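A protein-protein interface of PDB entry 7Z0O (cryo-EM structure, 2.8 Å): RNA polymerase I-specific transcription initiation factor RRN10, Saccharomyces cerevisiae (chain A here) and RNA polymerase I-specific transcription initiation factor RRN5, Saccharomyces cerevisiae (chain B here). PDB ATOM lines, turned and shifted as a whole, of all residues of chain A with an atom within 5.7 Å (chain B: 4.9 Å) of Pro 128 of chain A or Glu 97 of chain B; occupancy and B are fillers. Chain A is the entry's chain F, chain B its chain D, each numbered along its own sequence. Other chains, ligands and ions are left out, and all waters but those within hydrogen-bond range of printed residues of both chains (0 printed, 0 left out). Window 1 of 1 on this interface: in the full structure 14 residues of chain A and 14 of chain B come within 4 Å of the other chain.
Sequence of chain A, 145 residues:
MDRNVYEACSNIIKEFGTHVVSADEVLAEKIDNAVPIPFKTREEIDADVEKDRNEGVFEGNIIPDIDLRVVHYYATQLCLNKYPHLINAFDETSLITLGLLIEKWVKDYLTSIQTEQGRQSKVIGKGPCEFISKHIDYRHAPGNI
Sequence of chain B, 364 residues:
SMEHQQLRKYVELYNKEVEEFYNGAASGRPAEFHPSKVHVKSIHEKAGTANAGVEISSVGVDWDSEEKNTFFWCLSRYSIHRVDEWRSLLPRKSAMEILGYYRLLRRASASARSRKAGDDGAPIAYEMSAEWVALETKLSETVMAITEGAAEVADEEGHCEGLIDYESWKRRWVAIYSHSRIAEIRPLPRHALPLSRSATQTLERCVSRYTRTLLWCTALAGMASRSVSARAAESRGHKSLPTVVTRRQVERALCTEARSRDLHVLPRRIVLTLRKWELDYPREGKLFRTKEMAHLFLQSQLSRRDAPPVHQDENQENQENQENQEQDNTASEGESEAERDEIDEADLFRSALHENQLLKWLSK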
ATOM      1  N   TYR A 109      11.820  -5.753 -10.207  1.00  0.00           N
ATOM      2  CA  TYR A 109      13.171  -5.327  -9.861  1.00  0.00           C
ATOM      3  C   TYR A 109      13.586  -5.720  -8.459  1.00  0.00           C
ATOM      4  O   TYR A 109      14.672  -5.315  -8.040  1.00  0.00           O
ATOM      5  CB  TYR A 109      13.289  -3.813 -10.027  1.00  0.00           C
ATOM      6  CG  TYR A 109      13.353  -3.371 -11.465  1.00  0.00           C
ATOM      7  CD1 TYR A 109      14.534  -3.456 -12.184  1.00  0.00           C
ATOM      8  CD2 TYR A 109      12.230  -2.878 -12.109  1.00  0.00           C
ATOM      9  CE1 TYR A 109      14.596  -3.057 -13.500  1.00  0.00           C
ATOM     10  CE2 TYR A 109      12.283  -2.475 -13.425  1.00  0.00           C
ATOM     11  CZ  TYR A 109      13.467  -2.566 -14.116  1.00  0.00           C
ATOM     12  OH  TYR A 109      13.524  -2.167 -15.429  1.00  0.00           O
ATOM     13  N   LEU A 110      12.799  -6.480  -7.699  1.00  0.00           N
ATOM     14  CA  LEU A 110      13.162  -6.819  -6.335  1.00  0.00           C
ATOM     15  C   LEU A 110      13.091  -8.308  -6.033  1.00  0.00           C
ATOM     16  O   LEU A 110      13.581  -8.729  -4.981  1.00  0.00           O
ATOM     17  CB  LEU A 110      12.262  -6.069  -5.341  1.00  0.00           C
ATOM     18  CG  LEU A 110      12.339  -4.545  -5.340  1.00  0.00           C
ATOM     19  CD1 LEU A 110      11.187  -3.970  -4.541  1.00  0.00           C
ATOM     20  CD2 LEU A 110      13.668  -4.074  -4.782  1.00  0.00           C
ATOM     21  N   SER A 112      13.737 -12.485  -6.540  1.00  0.00           N
ATOM     22  CA  SER A 112      14.829 -13.373  -6.902  1.00  0.00           C
ATOM     23  C   SER A 112      14.431 -14.807  -6.588  1.00  0.00           C
ATOM     24  O   SER A 112      13.523 -15.059  -5.792  1.00  0.00           O
ATOM     25  CB  SER A 112      16.123 -13.006  -6.165  1.00  0.00           C
ATOM     26  OG  SER A 112      15.888 -12.853  -4.776  1.00  0.00           O
ATOM     27  N   ILE A 124      10.817 -11.910  -2.665  1.00  0.00           N
ATOM     28  CA  ILE A 124      11.774 -10.922  -2.177  1.00  0.00           C
ATOM     29  C   ILE A 124      12.431 -11.497  -0.924  1.00  0.00           C
ATOM     30  O   ILE A 124      11.742 -11.860   0.034  1.00  0.00           O
ATOM     31  CB  ILE A 124      11.100  -9.579  -1.883  1.00  0.00           C
ATOM     32  CG1 ILE A 124      10.364  -9.069  -3.122  1.00  0.00           C
ATOM     33  CG2 ILE A 124      12.128  -8.561  -1.421  1.00  0.00           C
ATOM     34  CD1 ILE A 124       9.867  -7.649  -2.992  1.00  0.00           C
ATOM     35  N   GLY A 125      13.756 -11.587  -0.925  1.00  0.00           N
ATOM     36  CA  GLY A 125      14.469 -12.224   0.158  1.00  0.00           C
ATOM     37  C   GLY A 125      15.458 -11.304   0.849  1.00  0.00           C
ATOM     38  O   GLY A 125      15.261 -10.096   0.984  1.00  0.00           O
ATOM     39  N   LYS A 126      16.554 -11.918   1.299  1.00  0.00           N
ATOM     40  CA  LYS A 126      17.631 -11.230   2.000  1.00  0.00           C
ATOM     41  C   LYS A 126      18.147 -10.002   1.265  1.00  0.00           C
ATOM     42  O   LYS A 126      18.259  -8.935   1.876  1.00  0.00           O
ATOM     43  CB  LYS A 126      18.803 -12.196   2.213  1.00  0.00           C
ATOM     44  CG  LYS A 126      18.769 -13.090   3.454  1.00  0.00           C
ATOM     45  CD  LYS A 126      18.689 -12.315   4.761  1.00  0.00           C
ATOM     46  CE  LYS A 126      17.282 -12.212   5.309  1.00  0.00           C
ATOM     47  NZ  LYS A 126      17.276 -11.644   6.684  1.00  0.00           N
ATOM     48  N   GLY A 127      18.441 -10.128  -0.026  1.00  0.00           N
ATOM     49  CA  GLY A 127      19.266  -9.186  -0.744  1.00  0.00           C
ATOM     50  C   GLY A 127      18.903  -7.719  -0.624  1.00  0.00           C
ATOM     51  O   GLY A 127      19.638  -6.928  -0.026  1.00  0.00           O
ATOM     52  N   PRO A 128      17.765  -7.322  -1.201  1.00  0.00           N
ATOM     53  CA  PRO A 128      17.444  -5.888  -1.257  1.00  0.00           C
ATOM     54  C   PRO A 128      17.351  -5.229   0.105  1.00  0.00           C
ATOM     55  O   PRO A 128      17.663  -4.039   0.227  1.00  0.00           O
ATOM     56  CB  PRO A 128      16.096  -5.864  -1.990  1.00  0.00           C
ATOM     57  CG  PRO A 128      16.074  -7.125  -2.773  1.00  0.00           C
ATOM     58  CD  PRO A 128      16.760  -8.132  -1.906  1.00  0.00           C
ATOM     59  N   CYS A 129      16.927  -5.961   1.136  1.00  0.00           N
ATOM     60  CA  CYS A 129      16.836  -5.375   2.469  1.00  0.00           C
ATOM     61  C   CYS A 129      18.220  -5.086   3.039  1.00  0.00           C
ATOM     62  O   CYS A 129      18.481  -3.984   3.535  1.00  0.00           O
ATOM     63  CB  CYS A 129      16.051  -6.304   3.394  1.00  0.00           C
ATOM     64  SG  CYS A 129      14.682  -7.165   2.590  1.00  0.00           S
ATOM     65  N   GLU A 130      19.125  -6.066   2.973  1.00  0.00           N
ATOM     66  CA  GLU A 130      20.465  -5.873   3.520  1.00  0.00           C
ATOM     67  C   GLU A 130      21.287  -4.895   2.695  1.00  0.00           C
ATOM     68  O   GLU A 130      22.189  -4.245   3.231  1.00  0.00           O
ATOM     69  CB  GLU A 130      21.193  -7.213   3.626  1.00  0.00           C
ATOM     70  CG  GLU A 130      20.955  -7.981   4.926  1.00  0.00           C
ATOM     71  CD  GLU A 130      19.546  -8.526   5.093  1.00  0.00           C
ATOM     72  OE1 GLU A 130      19.390  -9.495   5.864  1.00  0.00           O
ATOM     73  OE2 GLU A 130      18.597  -8.010   4.470  1.00  0.00           O
ATOM     74  N   PHE A 131      20.996  -4.775   1.399  1.00  0.00           N
ATOM     75  CA  PHE A 131      21.767  -3.872   0.554  1.00  0.00           C
ATOM     76  C   PHE A 131      21.621  -2.423   0.999  1.00  0.00           C
ATOM     77  O   PHE A 131      22.499  -1.598   0.728  1.00  0.00           O
ATOM     78  CB  PHE A 131      21.339  -4.030  -0.903  1.00  0.00           C
ATOM     79  CG  PHE A 131      22.104  -3.165  -1.852  1.00  0.00           C
ATOM     80  CD1 PHE A 131      23.423  -3.447  -2.153  1.00  0.00           C
ATOM     81  CD2 PHE A 131      21.508  -2.067  -2.440  1.00  0.00           C
ATOM     82  CE1 PHE A 131      24.133  -2.650  -3.025  1.00  0.00           C
ATOM     83  CE2 PHE A 131      22.212  -1.266  -3.312  1.00  0.00           C
ATOM     84  CZ  PHE A 131      23.526  -1.557  -3.605  1.00  0.00           C
ATOM     85  N   ILE A 132      20.528  -2.094   1.682  1.00  0.00           N
ATOM     86  CA  ILE A 132      20.303  -0.741   2.174  1.00  0.00           C
ATOM     87  C   ILE A 132      20.090  -0.790   3.680  1.00  0.00           C
ATOM     88  O   ILE A 132      19.427   0.081   4.254  1.00  0.00           O
ATOM     89  CB  ILE A 132      19.109  -0.083   1.464  1.00  0.00           C
ATOM     90  CG1 ILE A 132      17.855  -0.938   1.633  1.00  0.00           C
ATOM     91  CG2 ILE A 132      19.410   0.114  -0.007  1.00  0.00           C
ATOM     92  CD1 ILE A 132      16.593  -0.257   1.172  1.00  0.00           C
ATOM     93  N   SER A 133      20.656  -1.803   4.329  1.00  0.00           N
ATOM     94  CA  SER A 133      20.441  -2.011   5.750  1.00  0.00           C
ATOM     95  C   SER A 133      21.186  -0.964   6.574  1.00  0.00           C
ATOM     96  O   SER A 133      22.116  -0.302   6.108  1.00  0.00           O
ATOM     97  CB  SER A 133      20.893  -3.410   6.162  1.00  0.00           C
ATOM     98  OG  SER A 133      22.297  -3.545   6.029  1.00  0.00           O
ATOM     99  N   VAL B  61      25.001  -6.980   1.405  1.00  0.00           N
ATOM    100  CA  VAL B  61      24.520  -8.245   0.865  1.00  0.00           C
ATOM    101  C   VAL B  61      25.717  -9.072   0.420  1.00  0.00           C
ATOM    102  O   VAL B  61      26.708  -8.532  -0.083  1.00  0.00           O
ATOM    103  CB  VAL B  61      23.522  -8.015  -0.290  1.00  0.00           C
ATOM    104  CG1 VAL B  61      24.190  -7.308  -1.454  1.00  0.00           C
ATOM    105  CG2 VAL B  61      22.906  -9.326  -0.738  1.00  0.00           C
ATOM    106  N   TRP B  63      28.089 -11.198  -1.707  1.00  0.00           N
ATOM    107  CA  TRP B  63      28.424 -11.413  -3.108  1.00  0.00           C
ATOM    108  C   TRP B  63      29.529 -12.459  -3.160  1.00  0.00           C
ATOM    109  O   TRP B  63      30.694 -12.151  -2.891  1.00  0.00           O
ATOM    110  CB  TRP B  63      28.867 -10.114  -3.776  1.00  0.00           C
ATOM    111  CG  TRP B  63      27.761  -9.368  -4.458  1.00  0.00           C
ATOM    112  CD1 TRP B  63      26.874  -8.510  -3.880  1.00  0.00           C
ATOM    113  CD2 TRP B  63      27.431  -9.409  -5.850  1.00  0.00           C
ATOM    114  NE1 TRP B  63      26.011  -8.014  -4.824  1.00  0.00           N
ATOM    115  CE2 TRP B  63      26.331  -8.552  -6.042  1.00  0.00           C
ATOM    116  CE3 TRP B  63      27.955 -10.087  -6.951  1.00  0.00           C
ATOM    117  CZ2 TRP B  63      25.750  -8.357  -7.289  1.00  0.00           C
ATOM    118  CZ3 TRP B  63      27.377  -9.893  -8.186  1.00  0.00           C
ATOM    119  CH2 TRP B  63      26.286  -9.035  -8.346  1.00  0.00           C
ATOM    120  N   ARG B  92      20.152 -15.648  -7.083  1.00  0.00           N
ATOM    121  CA  ARG B  92      19.839 -15.117  -5.764  1.00  0.00           C
ATOM    122  C   ARG B  92      20.000 -13.607  -5.677  1.00  0.00           C
ATOM    123  O   ARG B  92      19.820 -13.043  -4.594  1.00  0.00           O
ATOM    124  CB  ARG B  92      20.715 -15.793  -4.706  1.00  0.00           C
ATOM    125  CG  ARG B  92      20.669 -17.310  -4.750  1.00  0.00           C
ATOM    126  CD  ARG B  92      21.390 -17.922  -3.563  1.00  0.00           C
ATOM    127  NE  ARG B  92      22.681 -17.288  -3.322  1.00  0.00           N
ATOM    128  CZ  ARG B  92      23.779 -17.532  -4.022  1.00  0.00           C
ATOM    129  NH1 ARG B  92      23.784 -18.398  -5.022  1.00  0.00           N
ATOM    130  NH2 ARG B  92      24.902 -16.890  -3.712  1.00  0.00           N
ATOM    131  N   LYS B  93      20.332 -12.944  -6.779  1.00  0.00           N
ATOM    132  CA  LYS B  93      20.516 -11.500  -6.810  1.00  0.00           C
ATOM    133  C   LYS B  93      19.391 -10.878  -7.622  1.00  0.00           C
ATOM    134  O   LYS B  93      19.192 -11.234  -8.788  1.00  0.00           O
ATOM    135  CB  LYS B  93      21.875 -11.137  -7.409  1.00  0.00           C
ATOM    136  CG  LYS B  93      23.054 -11.432  -6.504  1.00  0.00           C
ATOM    137  CD  LYS B  93      23.097 -10.470  -5.335  1.00  0.00           C
ATOM    138  CE  LYS B  93      24.233 -10.807  -4.392  1.00  0.00           C
ATOM    139  NZ  LYS B  93      23.968 -12.060  -3.640  1.00  0.00           N
ATOM    140  N   SER B  94      18.661  -9.953  -7.009  1.00  0.00           N
ATOM    141  CA  SER B  94      17.615  -9.230  -7.708  1.00  0.00           C
ATOM    142  C   SER B  94      18.224  -8.149  -8.594  1.00  0.00           C
ATOM    143  O   SER B  94      19.406  -7.816  -8.493  1.00  0.00           O
ATOM    144  CB  SER B  94      16.633  -8.618  -6.715  1.00  0.00           C
ATOM    145  OG  SER B  94      17.302  -7.780  -5.792  1.00  0.00           O
ATOM    146  N   ALA B  95      17.393  -7.596  -9.481  1.00  0.00           N
ATOM    147  CA  ALA B  95      17.871  -6.563 -10.394  1.00  0.00           C
ATOM    148  C   ALA B  95      18.315  -5.312  -9.650  1.00  0.00           C
ATOM    149  O   ALA B  95      19.187  -4.583 -10.134  1.00  0.00           O
ATOM    150  CB  ALA B  95      16.786  -6.219 -11.413  1.00  0.00           C
ATOM    151  N   MET B  96      17.725  -5.040  -8.485  1.00  0.00           N
ATOM    152  CA  MET B  96      18.160  -3.899  -7.686  1.00  0.00           C
ATOM    153  C   MET B  96      19.589  -4.087  -7.196  1.00  0.00           C
ATOM    154  O   MET B  96      20.404  -3.160  -7.249  1.00  0.00           O
ATOM    155  CB  MET B  96      17.214  -3.695  -6.505  1.00  0.00           C
ATOM    156  CG  MET B  96      17.687  -2.635  -5.526  1.00  0.00           C
ATOM    157  SD  MET B  96      17.431  -3.098  -3.805  1.00  0.00           S
ATOM    158  CE  MET B  96      17.546  -1.506  -3.000  1.00  0.00           C
ATOM    159  N   GLU B  97      19.909  -5.286  -6.707  1.00  0.00           N
ATOM    160  CA  GLU B  97      21.252  -5.545  -6.202  1.00  0.00           C
ATOM    161  C   GLU B  97      22.286  -5.495  -7.319  1.00  0.00           C
ATOM    162  O   GLU B  97      23.388  -4.970  -7.125  1.00  0.00           O
ATOM    163  CB  GLU B  97      21.293  -6.898  -5.496  1.00  0.00           C
ATOM    164  CG  GLU B  97      20.372  -6.994  -4.298  1.00  0.00           C
ATOM    165  CD  GLU B  97      19.951  -8.417  -4.008  1.00  0.00           C
ATOM    166  OE1 GLU B  97      20.780  -9.185  -3.485  1.00  0.00           O
ATOM    167  OE2 GLU B  97      18.793  -8.770  -4.303  1.00  0.00           O
ATOM    168  N   ILE B  98      21.956  -6.044  -8.488  1.00  0.00           N
ATOM    169  CA  ILE B  98      22.898  -6.035  -9.602  1.00  0.00           C
ATOM    170  C   ILE B  98      23.120  -4.614 -10.102  1.00  0.00           C
ATOM    171  O   ILE B  98      24.259  -4.176 -10.293  1.00  0.00           O
ATOM    172  CB  ILE B  98      22.406  -6.957 -10.728  1.00  0.00           C
ATOM    173  CG1 ILE B  98      22.228  -8.379 -10.208  1.00  0.00           C
ATOM    174  CG2 ILE B  98      23.376  -6.932 -11.885  1.00  0.00           C
ATOM    175  CD1 ILE B  98      21.414  -9.258 -11.120  1.00  0.00           C
ATOM    176  N   LEU B  99      22.034  -3.873 -10.327  1.00  0.00           N
ATOM    177  CA  LEU B  99      22.169  -2.486 -10.756  1.00  0.00           C
ATOM    178  C   LEU B  99      22.760  -1.628  -9.648  1.00  0.00           C
ATOM    179  O   LEU B  99      23.487  -0.667  -9.921  1.00  0.00           O
ATOM    180  CB  LEU B  99      20.815  -1.934 -11.197  1.00  0.00           C
ATOM    181  CG  LEU B  99      20.265  -2.457 -12.523  1.00  0.00           C
ATOM    182  CD1 LEU B  99      18.794  -2.111 -12.660  1.00  0.00           C
ATOM    183  CD2 LEU B  99      21.057  -1.901 -13.690  1.00  0.00           C
ATOM    184  N   GLY B 100      22.446  -1.951  -8.392  1.00  0.00           N
ATOM    185  CA  GLY B 100      23.046  -1.230  -7.283  1.00  0.00           C
ATOM    186  C   GLY B 100      24.548  -1.414  -7.220  1.00  0.00           C
ATOM    187  O   GLY B 100      25.290  -0.455  -6.998  1.00  0.00           O
ATOM    188  N   TYR B 101      25.018  -2.648  -7.424  1.00  0.00           N
ATOM    189  CA  TYR B 101      26.454  -2.904  -7.433  1.00  0.00           C
ATOM    190  C   TYR B 101      27.138  -2.154  -8.566  1.00  0.00           C
ATOM    191  O   TYR B 101      28.246  -1.633  -8.396  1.00  0.00           O
ATOM    192  CB  TYR B 101      26.715  -4.404  -7.548  1.00  0.00           C
ATOM    193  CG  TYR B 101      28.132  -4.809  -7.221  1.00  0.00           C
ATOM    194  CD1 TYR B 101      28.906  -4.057  -6.353  1.00  0.00           C
ATOM    195  CD2 TYR B 101      28.691  -5.948  -7.775  1.00  0.00           C
ATOM    196  CE1 TYR B 101      30.199  -4.425  -6.051  1.00  0.00           C
ATOM    197  CE2 TYR B 101      29.983  -6.325  -7.477  1.00  0.00           C
ATOM    198  CZ  TYR B 101      30.731  -5.561  -6.614  1.00  0.00           C
ATOM    199  OH  TYR B 101      32.020  -5.933  -6.315  1.00  0.00           O
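The backbone NH (N) of Met 96 of chain B lies within hydrogen-bond range of the backbone carbonyl oxygen (O) of Tyr 109 of chain A (3.1 Å).
The side-chain carboxylate of Glu 97 of chain B lies within hydrogen-bond range of the backbone NH of Ser 94 of chain B.
CD1 of Tyr 109 of chain A touches CB of Ala 95 of chain B, at 3.6 Å.
O of Leu 110 of chain A touches CB of Ser 94 of chain B, 3.5 Å away.
Leu 110 of chain A touches Met 96 of chain B (CD2 to CB, 3.96 Å).
Arg 92 of chain B touches Ser 112 of chain A.
CA of Gly 127 of chain A touches CG2 of Val 61 of chain B (3.6 Å).
Gly 127 of chain A touches Glu 97 of chain B (CA to OE1, 3.1 Å).
Ser 94 of chain B touches Pro 128 of chain A (OG to CG, 3.3 Å).
Pro 128 of chain A touches Met 96 of chain B.
Phe 131 of chain A touches Val 61 of chain B (CD1 to CG1, 3.998 Å).
Gly 100 of chain B touches Phe 131 of chain A (CA to CZ, 3.7 Å).
Pro 128 of chain A touches just these residues of chain B: Ser 94 (3.3 Å), Met 96 (3.6 Å) and Glu 97 (3.2 Å).
Glu 97 of chain B touches just these residues of chain A: Gly 127 (3.1 Å) and Pro 128 (3.2 Å).
Of the printed residues of chain A, Arg 92 of chain B touches Ser 112.
Of the printed residues of chain B, Phe 131 of chain A touches Val 61 (3.998 Å) and Gly 100 (3.7 Å).
Ile 124 of chain A touches none of the printed residues of chain B.
The nearest printed residue of chain B that does not touch Ile 132 of chain A is Val 61 of chain B (6.6 Å).
Printed residues of chain B that touch a printed residue of chain A: Val 61, Arg 92, Ser 94, Ala 95, Met 96, Glu 97 and Gly 100.
Of the 13 printed residues of chain A, 7 touch a printed residue of chain B.
Hydrophobic or aromatic side chains of chain A that line the printed part of chain B: Tyr 109, Leu 110, Pro 128, Phe 131 and Ile 132.
Among the printed residues, 13 pairs touch across the chains.
Among the printed residues, no Asp or Glu carboxylate lies within 4 Å of a Lys or Arg side-chain nitrogen of the other chain.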
